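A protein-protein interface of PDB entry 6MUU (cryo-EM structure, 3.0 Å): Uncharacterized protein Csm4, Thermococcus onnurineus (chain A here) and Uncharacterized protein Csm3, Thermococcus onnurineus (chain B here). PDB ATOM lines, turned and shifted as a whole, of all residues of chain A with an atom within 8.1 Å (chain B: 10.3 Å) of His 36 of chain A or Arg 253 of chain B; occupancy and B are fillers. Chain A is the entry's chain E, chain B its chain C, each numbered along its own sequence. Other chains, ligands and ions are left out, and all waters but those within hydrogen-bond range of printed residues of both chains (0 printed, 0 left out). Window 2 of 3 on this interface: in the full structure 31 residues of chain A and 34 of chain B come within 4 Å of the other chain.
The guanidinium group (NH2) of Arg 177 of chain A is in hydrogen-bond range of the backbone carbonyl oxygen (O) of Arg 253 of chain B (3.2 Å).
The backbone carbonyl oxygen of Tyr 252 of chain B sits at hydrogen-bond distance from the guanidinium group of Arg 177 of chain A (3.1 Å).
The guanidinium group of Arg 253 of chain B sits at hydrogen-bond distance from the backbone carbonyl oxygen of Ile 35 of chain A (2.9 Å).
The backbone carbonyl oxygen (O) of Ala 173 of chain A lies within hydrogen-bond range of the guanidinium group (NE) of Arg 177 of chain A (3.3 Å).
The side-chain carboxylate (OD1) of Asp 250 of chain B lies within salt-bridge range of the guanidinium group (NH1) of Arg 253 of chain B (3.6 Å).
Ala 34 of chain A touches Phe 6 of chain B (O to CB, 3.9 Å).
Ile 35 of chain A touches Tyr 252 of chain B (CD1 to CB, 3.9 Å).
His 36 of chain A touches Arg 253 of chain B (CE1 to NE, 3.97 Å).
Pro 174 of chain A touches Tyr 252 of chain B.
CA of Gly 255 of chain B touches NH1 of Arg 177 of chain A, 3.3 Å away.
Phe 6 of chain B touches Phe 178 of chain A.
CA of Phe 178 of chain A touches CD1 of Tyr 252 of chain B, at 3.8 Å.
No residue of chain B comes within 4 Å of Ile 32 of chain A.
Of the printed residues of chain B, Ala 34 of chain A touches Phe 6.
His 36 of chain A touches one residue of chain B.
No residue of chain B comes within 4 Å of Gly 37 of chain A.
Of chain B, only Tyr 252 comes within 4 Å of Pro 174 of chain A.
Arg 5 of chain B touches none of the printed residues of chain A.
Printed residues of chain A within 4 Å of Phe 6 of chain B: Ala 34 and Phe 178.
Printed residues of chain A within 4 Å of Tyr 252 of chain B: Ile 35 (3.9 Å), Pro 174 (3.6 Å), Arg 177 (3.1 Å) and Phe 178 (3.8 Å).
Of chain A, only Ile 35 (2.9 Å), His 36 (3.97 Å) and Arg 177 (3.2 Å) come within 4 Å of Arg 253 of chain B.
Of the printed residues of chain A, Gly 255 of chain B touches Arg 177.
The nearest printed residue of chain A that does not touch Phe 6 of chain B is Ile 35 of chain A (5.1 Å).
Of the 17 printed residues of chain B, 4 touch a printed residue of chain A.
Hydrophobic or aromatic side chains of chain B within 4 Å of the printed part of chain A: Phe 6 and Tyr 252.
Of the 21 printed residues of chain A, 6 touch a printed residue of chain B.
Printed residues of chain A that touch a printed residue of chain B: Ala 34, Ile 35, His 36, Pro 174, Arg 177 and Phe 178.
Hydrophobic or aromatic side chains of chain A that line the printed part of chain B: Ile 35, His 36, Pro 174 and Phe 178.
Among the printed residues, no Asp or Glu carboxylate lies within 4 Å of a Lys or Arg side-chain nitrogen of the other chain.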
ATOM      1  N   ASN A  30      22.240  -5.071  -9.995  1.00  0.00           N
ATOM      2  CA  ASN A  30      21.505  -5.370  -8.772  1.00  0.00           C
ATOM      3  C   ASN A  30      22.351  -6.144  -7.778  1.00  0.00           C
ATOM      4  O   ASN A  30      22.116  -6.054  -6.570  1.00  0.00           O
ATOM      5  CB  ASN A  30      20.234  -6.154  -9.089  1.00  0.00           C
ATOM      6  CG  ASN A  30      19.154  -5.288  -9.664  1.00  0.00           C
ATOM      7  OD1 ASN A  30      18.808  -5.399 -10.829  1.00  0.00           O
ATOM      8  ND2 ASN A  30      18.602  -4.419  -8.839  1.00  0.00           N
ATOM      9  N   ALA A  31      23.328  -6.913  -8.255  1.00  0.00           N
ATOM     10  CA  ALA A  31      24.167  -7.677  -7.346  1.00  0.00           C
ATOM     11  C   ALA A  31      25.189  -6.802  -6.641  1.00  0.00           C
ATOM     12  O   ALA A  31      25.615  -7.128  -5.533  1.00  0.00           O
ATOM     13  CB  ALA A  31      24.872  -8.796  -8.102  1.00  0.00           C
ATOM     14  N   ILE A  32      25.585  -5.692  -7.254  1.00  0.00           N
ATOM     15  CA  ILE A  32      26.617  -4.854  -6.661  1.00  0.00           C
ATOM     16  C   ILE A  32      26.030  -3.955  -5.588  1.00  0.00           C
ATOM     17  O   ILE A  32      26.627  -3.771  -4.523  1.00  0.00           O
ATOM     18  CB  ILE A  32      27.331  -4.064  -7.770  1.00  0.00           C
ATOM     19  CG1 ILE A  32      28.065  -5.028  -8.692  1.00  0.00           C
ATOM     20  CG2 ILE A  32      28.307  -3.075  -7.211  1.00  0.00           C
ATOM     21  CD1 ILE A  32      29.093  -5.864  -7.991  1.00  0.00           C
ATOM     22  N   SER A  33      24.836  -3.416  -5.823  1.00  0.00           N
ATOM     23  CA  SER A  33      24.191  -2.587  -4.816  1.00  0.00           C
ATOM     24  C   SER A  33      23.706  -3.396  -3.625  1.00  0.00           C
ATOM     25  O   SER A  33      23.545  -2.836  -2.539  1.00  0.00           O
ATOM     26  CB  SER A  33      23.027  -1.824  -5.434  1.00  0.00           C
ATOM     27  OG  SER A  33      22.029  -2.717  -5.878  1.00  0.00           O
ATOM     28  N   ALA A  34      23.473  -4.693  -3.796  1.00  0.00           N
ATOM     29  CA  ALA A  34      23.140  -5.532  -2.654  1.00  0.00           C
ATOM     30  C   ALA A  34      24.378  -5.839  -1.824  1.00  0.00           C
ATOM     31  O   ALA A  34      24.349  -5.748  -0.594  1.00  0.00           O
ATOM     32  CB  ALA A  34      22.473  -6.822  -3.123  1.00  0.00           C
ATOM     33  N   ILE A  35      25.476  -6.193  -2.484  1.00  0.00           N
ATOM     34  CA  ILE A  35      26.695  -6.556  -1.770  1.00  0.00           C
ATOM     35  C   ILE A  35      27.402  -5.315  -1.244  1.00  0.00           C
ATOM     36  O   ILE A  35      27.651  -5.184  -0.042  1.00  0.00           O
ATOM     37  CB  ILE A  35      27.622  -7.383  -2.676  1.00  0.00           C
ATOM     38  CG1 ILE A  35      26.980  -8.715  -3.026  1.00  0.00           C
ATOM     39  CG2 ILE A  35      28.943  -7.618  -2.002  1.00  0.00           C
ATOM     40  CD1 ILE A  35      27.721  -9.441  -4.101  1.00  0.00           C
ATOM     41  N   HIS A  36      27.735  -4.385  -2.136  1.00  0.00           N
ATOM     42  CA  HIS A  36      28.522  -3.211  -1.745  1.00  0.00           C
ATOM     43  C   HIS A  36      27.626  -2.023  -1.407  1.00  0.00           C
ATOM     44  O   HIS A  36      27.616  -1.547  -0.269  1.00  0.00           O
ATOM     45  CB  HIS A  36      29.508  -2.850  -2.852  1.00  0.00           C
ATOM     46  CG  HIS A  36      30.556  -3.888  -3.085  1.00  0.00           C
ATOM     47  ND1 HIS A  36      31.601  -4.093  -2.213  1.00  0.00           N
ATOM     48  CD2 HIS A  36      30.728  -4.773  -4.094  1.00  0.00           C
ATOM     49  CE1 HIS A  36      32.368  -5.065  -2.672  1.00  0.00           C
ATOM     50  NE2 HIS A  36      31.862  -5.493  -3.813  1.00  0.00           N
ATOM     51  N   GLY A  37      26.872  -1.547  -2.376  1.00  0.00           N
ATOM     52  CA  GLY A  37      26.034  -0.384  -2.170  1.00  0.00           C
ATOM     53  C   GLY A  37      25.961   0.445  -3.434  1.00  0.00           C
ATOM     54  O   GLY A  37      26.505   0.089  -4.470  1.00  0.00           O
ATOM     55  N   GLN A  38      25.278   1.581  -3.313  1.00  0.00           N
ATOM     56  CA  GLN A  38      24.974   2.408  -4.473  1.00  0.00           C
ATOM     57  C   GLN A  38      26.184   3.165  -4.995  1.00  0.00           C
ATOM     58  O   GLN A  38      26.199   3.539  -6.172  1.00  0.00           O
ATOM     59  CB  GLN A  38      23.851   3.392  -4.134  1.00  0.00           C
ATOM     60  CG  GLN A  38      24.226   4.530  -3.187  1.00  0.00           C
ATOM     61  CD  GLN A  38      24.110   4.158  -1.716  1.00  0.00           C
ATOM     62  OE1 GLN A  38      24.061   2.982  -1.357  1.00  0.00           O
ATOM     63  NE2 GLN A  38      24.058   5.168  -0.859  1.00  0.00           N
ATOM     64  N   SER A  39      27.195   3.396  -4.157  1.00  0.00           N
ATOM     65  CA  SER A  39      28.398   4.079  -4.606  1.00  0.00           C
ATOM     66  C   SER A  39      29.255   3.200  -5.500  1.00  0.00           C
ATOM     67  O   SER A  39      30.023   3.724  -6.311  1.00  0.00           O
ATOM     68  CB  SER A  39      29.214   4.541  -3.404  1.00  0.00           C
ATOM     69  OG  SER A  39      29.686   3.427  -2.671  1.00  0.00           O
ATOM     70  N   ALA A  40      29.144   1.880  -5.365  1.00  0.00           N
ATOM     71  CA  ALA A  40      29.894   0.973  -6.219  1.00  0.00           C
ATOM     72  C   ALA A  40      29.209   0.718  -7.551  1.00  0.00           C
ATOM     73  O   ALA A  40      29.873   0.292  -8.498  1.00  0.00           O
ATOM     74  CB  ALA A  40      30.135  -0.349  -5.498  1.00  0.00           C
ATOM     75  N   VAL A  41      27.902   0.960  -7.650  1.00  0.00           N
ATOM     76  CA  VAL A  41      27.260   0.903  -8.958  1.00  0.00           C
ATOM     77  C   VAL A  41      27.691   2.098  -9.800  1.00  0.00           C
ATOM     78  O   VAL A  41      27.864   1.981 -11.020  1.00  0.00           O
ATOM     79  CB  VAL A  41      25.730   0.824  -8.797  1.00  0.00           C
ATOM     80  CG1 VAL A  41      25.034   0.764 -10.138  1.00  0.00           C
ATOM     81  CG2 VAL A  41      25.354  -0.378  -7.985  1.00  0.00           C
ATOM     82  N   ASP A 169      37.837  -8.532 -11.154  1.00  0.00           N
ATOM     83  CA  ASP A 169      38.074  -9.165  -9.867  1.00  0.00           C
ATOM     84  C   ASP A 169      37.243  -8.535  -8.758  1.00  0.00           C
ATOM     85  O   ASP A 169      36.983  -9.188  -7.744  1.00  0.00           O
ATOM     86  CB  ASP A 169      39.565  -9.074  -9.529  1.00  0.00           C
ATOM     87  CG  ASP A 169      40.006 -10.101  -8.505  1.00  0.00           C
ATOM     88  OD1 ASP A 169      39.183 -10.935  -8.078  1.00  0.00           O
ATOM     89  OD2 ASP A 169      41.199 -10.078  -8.134  1.00  0.00           O
ATOM     90  N   GLY A 170      36.807  -7.293  -8.935  1.00  0.00           N
ATOM     91  CA  GLY A 170      36.095  -6.601  -7.884  1.00  0.00           C
ATOM     92  C   GLY A 170      34.609  -6.457  -8.125  1.00  0.00           C
ATOM     93  O   GLY A 170      33.845  -6.293  -7.172  1.00  0.00           O
ATOM     94  N   TYR A 171      34.177  -6.506  -9.384  1.00  0.00           N
ATOM     95  CA  TYR A 171      32.779  -6.256  -9.700  1.00  0.00           C
ATOM     96  C   TYR A 171      32.084  -7.442 -10.343  1.00  0.00           C
ATOM     97  O   TYR A 171      31.039  -7.873  -9.852  1.00  0.00           O
ATOM     98  CB  TYR A 171      32.653  -5.030 -10.610  1.00  0.00           C
ATOM     99  CG  TYR A 171      33.093  -3.746  -9.954  1.00  0.00           C
ATOM    100  CD1 TYR A 171      32.312  -3.138  -8.986  1.00  0.00           C
ATOM    101  CD2 TYR A 171      34.279  -3.131 -10.321  1.00  0.00           C
ATOM    102  CE1 TYR A 171      32.711  -1.968  -8.385  1.00  0.00           C
ATOM    103  CE2 TYR A 171      34.684  -1.956  -9.732  1.00  0.00           C
ATOM    104  CZ  TYR A 171      33.900  -1.380  -8.766  1.00  0.00           C
ATOM    105  OH  TYR A 171      34.309  -0.206  -8.180  1.00  0.00           O
ATOM    106  N   ILE A 172      32.631  -7.989 -11.424  1.00  0.00           N
ATOM    107  CA  ILE A 172      31.915  -9.030 -12.152  1.00  0.00           C
ATOM    108  C   ILE A 172      32.045 -10.373 -11.444  1.00  0.00           C
ATOM    109  O   ILE A 172      31.067 -11.115 -11.320  1.00  0.00           O
ATOM    110  CB  ILE A 172      32.385  -9.088 -13.620  1.00  0.00           C
ATOM    111  CG1 ILE A 172      31.936  -7.841 -14.385  1.00  0.00           C
ATOM    112  CG2 ILE A 172      31.834 -10.298 -14.337  1.00  0.00           C
ATOM    113  CD1 ILE A 172      32.964  -6.746 -14.486  1.00  0.00           C
ATOM    114  N   ALA A 173      33.217 -10.687 -10.914  1.00  0.00           N
ATOM    115  CA  ALA A 173      33.385 -11.939 -10.178  1.00  0.00           C
ATOM    116  C   ALA A 173      32.629 -12.027  -8.845  1.00  0.00           C
ATOM    117  O   ALA A 173      32.144 -13.119  -8.529  1.00  0.00           O
ATOM    118  CB  ALA A 173      34.871 -12.232  -9.954  1.00  0.00           C
ATOM    119  N   PRO A 174      32.486 -10.968  -8.023  1.00  0.00           N
ATOM    120  CA  PRO A 174      31.578 -11.101  -6.874  1.00  0.00           C
ATOM    121  C   PRO A 174      30.118 -11.106  -7.249  1.00  0.00           C
ATOM    122  O   PRO A 174      29.305 -11.627  -6.480  1.00  0.00           O
ATOM    123  CB  PRO A 174      31.910  -9.881  -6.012  1.00  0.00           C
ATOM    124  CG  PRO A 174      33.234  -9.503  -6.396  1.00  0.00           C
ATOM    125  CD  PRO A 174      33.313  -9.760  -7.848  1.00  0.00           C
ATOM    126  N   ALA A 175      29.755 -10.529  -8.392  1.00  0.00           N
ATOM    127  CA  ALA A 175      28.357 -10.507  -8.789  1.00  0.00           C
ATOM    128  C   ALA A 175      27.873 -11.885  -9.194  1.00  0.00           C
ATOM    129  O   ALA A 175      26.719 -12.229  -8.936  1.00  0.00           O
ATOM    130  CB  ALA A 175      28.140  -9.526  -9.934  1.00  0.00           C
ATOM    131  N   ARG A 177      28.685 -14.789  -8.043  1.00  0.00           N
ATOM    132  CA  ARG A 177      28.433 -15.674  -6.915  1.00  0.00           C
ATOM    133  C   ARG A 177      27.157 -15.292  -6.185  1.00  0.00           C
ATOM    134  O   ARG A 177      26.489 -16.162  -5.623  1.00  0.00           O
ATOM    135  CB  ARG A 177      29.622 -15.648  -5.965  1.00  0.00           C
ATOM    136  CG  ARG A 177      30.870 -16.143  -6.639  1.00  0.00           C
ATOM    137  CD  ARG A 177      32.107 -15.965  -5.802  1.00  0.00           C
ATOM    138  NE  ARG A 177      32.347 -14.556  -5.524  1.00  0.00           N
ATOM    139  CZ  ARG A 177      33.436 -14.096  -4.929  1.00  0.00           C
ATOM    140  NH1 ARG A 177      34.409 -14.927  -4.609  1.00  0.00           N
ATOM    141  NH2 ARG A 177      33.573 -12.797  -4.701  1.00  0.00           N
ATOM    142  N   PHE A 178      26.806 -14.005  -6.184  1.00  0.00           N
ATOM    143  CA  PHE A 178      25.493 -13.594  -5.701  1.00  0.00           C
ATOM    144  C   PHE A 178      24.402 -14.034  -6.661  1.00  0.00           C
ATOM    145  O   PHE A 178      23.365 -14.546  -6.234  1.00  0.00           O
ATOM    146  CB  PHE A 178      25.455 -12.081  -5.520  1.00  0.00           C
ATOM    147  CG  PHE A 178      24.164 -11.560  -4.951  1.00  0.00           C
ATOM    148  CD1 PHE A 178      23.918 -11.617  -3.599  1.00  0.00           C
ATOM    149  CD2 PHE A 178      23.204 -10.996  -5.775  1.00  0.00           C
ATOM    150  CE1 PHE A 178      22.740 -11.134  -3.085  1.00  0.00           C
ATOM    151  CE2 PHE A 178      22.029 -10.509  -5.259  1.00  0.00           C
ATOM    152  CZ  PHE A 178      21.799 -10.576  -3.914  1.00  0.00           C
ATOM    153  N   ARG B   5      18.328  -4.283   0.599  1.00  0.00           N
ATOM    154  CA  ARG B   5      19.035  -4.608   1.830  1.00  0.00           C
ATOM    155  C   ARG B   5      19.268  -6.113   1.921  1.00  0.00           C
ATOM    156  O   ARG B   5      18.350  -6.898   1.711  1.00  0.00           O
ATOM    157  CB  ARG B   5      18.250  -4.102   3.034  1.00  0.00           C
ATOM    158  CG  ARG B   5      18.888  -4.376   4.378  1.00  0.00           C
ATOM    159  CD  ARG B   5      20.134  -3.537   4.624  1.00  0.00           C
ATOM    160  NE  ARG B   5      21.365  -4.211   4.222  1.00  0.00           N
ATOM    161  CZ  ARG B   5      22.566  -3.643   4.244  1.00  0.00           C
ATOM    162  NH1 ARG B   5      23.638  -4.325   3.867  1.00  0.00           N
ATOM    163  NH2 ARG B   5      22.695  -2.390   4.651  1.00  0.00           N
ATOM    164  N   PHE B   6      20.501  -6.509   2.237  1.00  0.00           N
ATOM    165  CA  PHE B   6      20.916  -7.899   2.117  1.00  0.00           C
ATOM    166  C   PHE B   6      21.920  -8.256   3.199  1.00  0.00           C
ATOM    167  O   PHE B   6      22.805  -7.462   3.518  1.00  0.00           O
ATOM    168  CB  PHE B   6      21.521  -8.156   0.738  1.00  0.00           C
ATOM    169  CG  PHE B   6      22.037  -9.540   0.557  1.00  0.00           C
ATOM    170  CD1 PHE B   6      21.165 -10.601   0.454  1.00  0.00           C
ATOM    171  CD2 PHE B   6      23.394  -9.781   0.471  1.00  0.00           C
ATOM    172  CE1 PHE B   6      21.636 -11.880   0.287  1.00  0.00           C
ATOM    173  CE2 PHE B   6      23.868 -11.059   0.298  1.00  0.00           C
ATOM    174  CZ  PHE B   6      22.987 -12.108   0.213  1.00  0.00           C
ATOM    175  N   TYR B   7      21.789  -9.471   3.738  1.00  0.00           N
ATOM    176  CA  TYR B   7      22.652  -9.959   4.806  1.00  0.00           C
ATOM    177  C   TYR B   7      23.220 -11.349   4.582  1.00  0.00           C
ATOM    178  O   TYR B   7      24.216 -11.687   5.225  1.00  0.00           O
ATOM    179  CB  TYR B   7      21.896  -9.973   6.139  1.00  0.00           C
ATOM    180  CG  TYR B   7      21.490  -8.610   6.624  1.00  0.00           C
ATOM    181  CD1 TYR B   7      22.380  -7.801   7.306  1.00  0.00           C
ATOM    182  CD2 TYR B   7      20.216  -8.128   6.382  1.00  0.00           C
ATOM    183  CE1 TYR B   7      22.006  -6.551   7.745  1.00  0.00           C
ATOM    184  CE2 TYR B   7      19.834  -6.887   6.815  1.00  0.00           C
ATOM    185  CZ  TYR B   7      20.730  -6.099   7.494  1.00  0.00           C
ATOM    186  OH  TYR B   7      20.342  -4.855   7.925  1.00  0.00           O
ATOM    187  N   GLY B   8      22.629 -12.168   3.731  1.00  0.00           N
ATOM    188  CA  GLY B   8      23.082 -13.530   3.546  1.00  0.00           C
ATOM    189  C   GLY B   8      21.938 -14.400   3.068  1.00  0.00           C
ATOM    190  O   GLY B   8      20.846 -13.917   2.802  1.00  0.00           O
ATOM    191  N   ARG B 247      26.070 -18.735   4.604  1.00  0.00           N
ATOM    192  CA  ARG B 247      26.594 -17.904   3.517  1.00  0.00           C
ATOM    193  C   ARG B 247      26.412 -16.416   3.788  1.00  0.00           C
ATOM    194  O   ARG B 247      25.513 -15.796   3.211  1.00  0.00           O
ATOM    195  CB  ARG B 247      25.936 -18.267   2.185  1.00  0.00           C
ATOM    196  CG  ARG B 247      26.253 -19.664   1.716  1.00  0.00           C
ATOM    197  CD  ARG B 247      25.665 -19.945   0.357  1.00  0.00           C
ATOM    198  NE  ARG B 247      25.905 -21.321  -0.060  1.00  0.00           N
ATOM    199  CZ  ARG B 247      25.460 -21.850  -1.196  1.00  0.00           C
ATOM    200  NH1 ARG B 247      24.750 -21.120  -2.039  1.00  0.00           N
ATOM    201  NH2 ARG B 247      25.724 -23.116  -1.485  1.00  0.00           N
ATOM    202  N   PRO B 248      27.207 -15.824   4.676  1.00  0.00           N
ATOM    203  CA  PRO B 248      26.959 -14.442   5.108  1.00  0.00           C
ATOM    204  C   PRO B 248      27.190 -13.387   4.044  1.00  0.00           C
ATOM    205  O   PRO B 248      27.574 -13.687   2.912  1.00  0.00           O
ATOM    206  CB  PRO B 248      27.952 -14.262   6.256  1.00  0.00           C
ATOM    207  CG  PRO B 248      29.045 -15.192   5.933  1.00  0.00           C
ATOM    208  CD  PRO B 248      28.415 -16.383   5.295  1.00  0.00           C
ATOM    209  N   LEU B 249      26.952 -12.131   4.431  1.00  0.00           N
ATOM    210  CA  LEU B 249      27.174 -10.996   3.541  1.00  0.00           C
ATOM    211  C   LEU B 249      28.644 -10.838   3.195  1.00  0.00           C
ATOM    212  O   LEU B 249      28.972 -10.337   2.116  1.00  0.00           O
ATOM    213  CB  LEU B 249      26.615  -9.724   4.190  1.00  0.00           C
ATOM    214  CG  LEU B 249      26.570  -8.318   3.570  1.00  0.00           C
ATOM    215  CD1 LEU B 249      27.833  -7.530   3.838  1.00  0.00           C
ATOM    216  CD2 LEU B 249      26.321  -8.377   2.082  1.00  0.00           C
ATOM    217  N   ASP B 250      29.538 -11.266   4.078  1.00  0.00           N
ATOM    218  CA  ASP B 250      30.953 -11.137   3.786  1.00  0.00           C
ATOM    219  C   ASP B 250      31.453 -12.243   2.869  1.00  0.00           C
ATOM    220  O   ASP B 250      32.487 -12.066   2.223  1.00  0.00           O
ATOM    221  CB  ASP B 250      31.757 -11.117   5.084  1.00  0.00           C
ATOM    222  CG  ASP B 250      33.182 -10.658   4.874  1.00  0.00           C
ATOM    223  OD1 ASP B 250      33.383  -9.450   4.635  1.00  0.00           O
ATOM    224  OD2 ASP B 250      34.099 -11.502   4.938  1.00  0.00           O
ATOM    225  N   TYR B 251      30.726 -13.362   2.781  1.00  0.00           N
ATOM    226  CA  TYR B 251      31.094 -14.443   1.869  1.00  0.00           C
ATOM    227  C   TYR B 251      31.021 -14.021   0.412  1.00  0.00           C
ATOM    228  O   TYR B 251      31.837 -14.465  -0.399  1.00  0.00           O
ATOM    229  CB  TYR B 251      30.183 -15.647   2.087  1.00  0.00           C
ATOM    230  CG  TYR B 251      30.378 -16.763   1.085  1.00  0.00           C
ATOM    231  CD1 TYR B 251      31.475 -17.603   1.158  1.00  0.00           C
ATOM    232  CD2 TYR B 251      29.454 -16.979   0.068  1.00  0.00           C
ATOM    233  CE1 TYR B 251      31.652 -18.621   0.245  1.00  0.00           C
ATOM    234  CE2 TYR B 251      29.626 -17.987  -0.850  1.00  0.00           C
ATOM    235  CZ  TYR B 251      30.722 -18.809  -0.753  1.00  0.00           C
ATOM    236  OH  TYR B 251      30.894 -19.819  -1.664  1.00  0.00           O
ATOM    237  N   TYR B 252      30.046 -13.191   0.056  1.00  0.00           N
ATOM    238  CA  TYR B 252      29.828 -12.882  -1.347  1.00  0.00           C
ATOM    239  C   TYR B 252      30.859 -11.922  -1.913  1.00  0.00           C
ATOM    240  O   TYR B 252      31.080 -11.928  -3.127  1.00  0.00           O
ATOM    241  CB  TYR B 252      28.417 -12.331  -1.549  1.00  0.00           C
ATOM    242  CG  TYR B 252      27.365 -13.389  -1.358  1.00  0.00           C
ATOM    243  CD1 TYR B 252      27.109 -14.315  -2.356  1.00  0.00           C
ATOM    244  CD2 TYR B 252      26.640 -13.474  -0.183  1.00  0.00           C
ATOM    245  CE1 TYR B 252      26.167 -15.292  -2.193  1.00  0.00           C
ATOM    246  CE2 TYR B 252      25.691 -14.446  -0.014  1.00  0.00           C
ATOM    247  CZ  TYR B 252      25.464 -15.353  -1.024  1.00  0.00           C
ATOM    248  OH  TYR B 252      24.522 -16.335  -0.873  1.00  0.00           O
ATOM    249  N   ARG B 253      31.518 -11.123  -1.083  1.00  0.00           N
ATOM    250  CA  ARG B 253      32.531 -10.255  -1.662  1.00  0.00           C
ATOM    251  C   ARG B 253      33.927 -10.870  -1.648  1.00  0.00           C
ATOM    252  O   ARG B 253      34.707 -10.624  -2.574  1.00  0.00           O
ATOM    253  CB  ARG B 253      32.541  -8.892  -0.966  1.00  0.00           C
ATOM    254  CG  ARG B 253      32.862  -8.909   0.509  1.00  0.00           C
ATOM    255  CD  ARG B 253      33.044  -7.500   1.017  1.00  0.00           C
ATOM    256  NE  ARG B 253      31.827  -6.712   0.899  1.00  0.00           N
ATOM    257  CZ  ARG B 253      30.922  -6.604   1.861  1.00  0.00           C
ATOM    258  NH1 ARG B 253      31.114  -7.224   3.014  1.00  0.00           N
ATOM    259  NH2 ARG B 253      29.843  -5.860   1.679  1.00  0.00           N
ATOM    260  N   THR B 254      34.276 -11.677  -0.645  1.00  0.00           N
ATOM    261  CA  THR B 254      35.636 -12.199  -0.600  1.00  0.00           C
ATOM    262  C   THR B 254      35.755 -13.647  -1.057  1.00  0.00           C
ATOM    263  O   THR B 254      36.835 -14.048  -1.497  1.00  0.00           O
ATOM    264  CB  THR B 254      36.243 -12.045   0.804  1.00  0.00           C
ATOM    265  OG1 THR B 254      37.642 -12.347   0.750  1.00  0.00           O
ATOM    266  CG2 THR B 254      35.591 -12.961   1.820  1.00  0.00           C
ATOM    267  N   GLY B 255      34.687 -14.439  -0.990  1.00  0.00           N
ATOM    268  CA  GLY B 255      34.729 -15.811  -1.449  1.00  0.00           C
ATOM    269  C   GLY B 255      35.346 -16.813  -0.501  1.00  0.00           C
ATOM    270  O   GLY B 255      35.333 -18.013  -0.804  1.00  0.00           O
ATOM    271  N   LYS B 256      35.893 -16.379   0.627  1.00  0.00           N
ATOM    272  CA  LYS B 256      36.471 -17.312   1.581  1.00  0.00           C
ATOM    273  C   LYS B 256      35.374 -17.913   2.449  1.00  0.00           C
ATOM    274  O   LYS B 256      34.322 -17.307   2.658  1.00  0.00           O
ATOM    275  CB  LYS B 256      37.522 -16.610   2.439  1.00  0.00           C
ATOM    276  CG  LYS B 256      38.676 -15.965   1.659  1.00  0.00           C
ATOM    277  CD  LYS B 256      39.678 -16.980   1.088  1.00  0.00           C
ATOM    278  CE  LYS B 256      39.505 -17.233  -0.415  1.00  0.00           C
ATOM    279  NZ  LYS B 256      40.555 -18.137  -0.952  1.00  0.00           N
ATOM    280  N   ASP B 257      35.630 -19.114   2.960  1.00  0.00           N
ATOM    281  CA  ASP B 257      34.597 -19.909   3.622  1.00  0.00           C
ATOM    282  C   ASP B 257      34.327 -19.365   5.019  1.00  0.00           C
ATOM    283  O   ASP B 257      34.889 -19.819   6.016  1.00  0.00           O
ATOM    284  CB  ASP B 257      34.998 -21.374   3.660  1.00  0.00           C
ATOM    285  CG  ASP B 257      34.941 -22.019   2.297  1.00  0.00           C
ATOM    286  OD1 ASP B 257      34.117 -21.575   1.470  1.00  0.00           O
ATOM    287  OD2 ASP B 257      35.718 -22.963   2.048  1.00  0.00           O
ATOM    288  N   GLU B 258      33.444 -18.370   5.078  1.00  0.00           N
ATOM    289  CA  GLU B 258      32.853 -17.890   6.317  1.00  0.00           C
ATOM    290  C   GLU B 258      31.473 -18.523   6.532  1.00  0.00           C
ATOM    291  O   GLU B 258      30.667 -18.031   7.329  1.00  0.00           O
ATOM    292  CB  GLU B 258      32.794 -16.355   6.282  1.00  0.00           C
ATOM    293  CG  GLU B 258      32.654 -15.619   7.626  1.00  0.00           C
ATOM    294  CD  GLU B 258      33.871 -15.781   8.522  1.00  0.00           C
ATOM    295  OE1 GLU B 258      34.987 -15.973   7.994  1.00  0.00           O
ATOM    296  OE2 GLU B 258      33.708 -15.717   9.760  1.00  0.00           O
ATOM    297  N   ASP B 259      31.200 -19.624   5.838  1.00  0.00           N
ATOM    298  CA  ASP B 259      29.888 -20.258   5.856  1.00  0.00           C
ATOM    299  C   ASP B 259      29.662 -20.937   7.199  1.00  0.00           C
ATOM    300  O   ASP B 259      30.319 -21.932   7.518  1.00  0.00           O
ATOM    301  CB  ASP B 259      29.785 -21.270   4.722  1.00  0.00           C
ATOM    302  CG  ASP B 259      29.974 -20.642   3.369  1.00  0.00           C
ATOM    303  OD1 ASP B 259      29.727 -19.432   3.245  1.00  0.00           O
ATOM    304  OD2 ASP B 259      30.360 -21.356   2.423  1.00  0.00           O
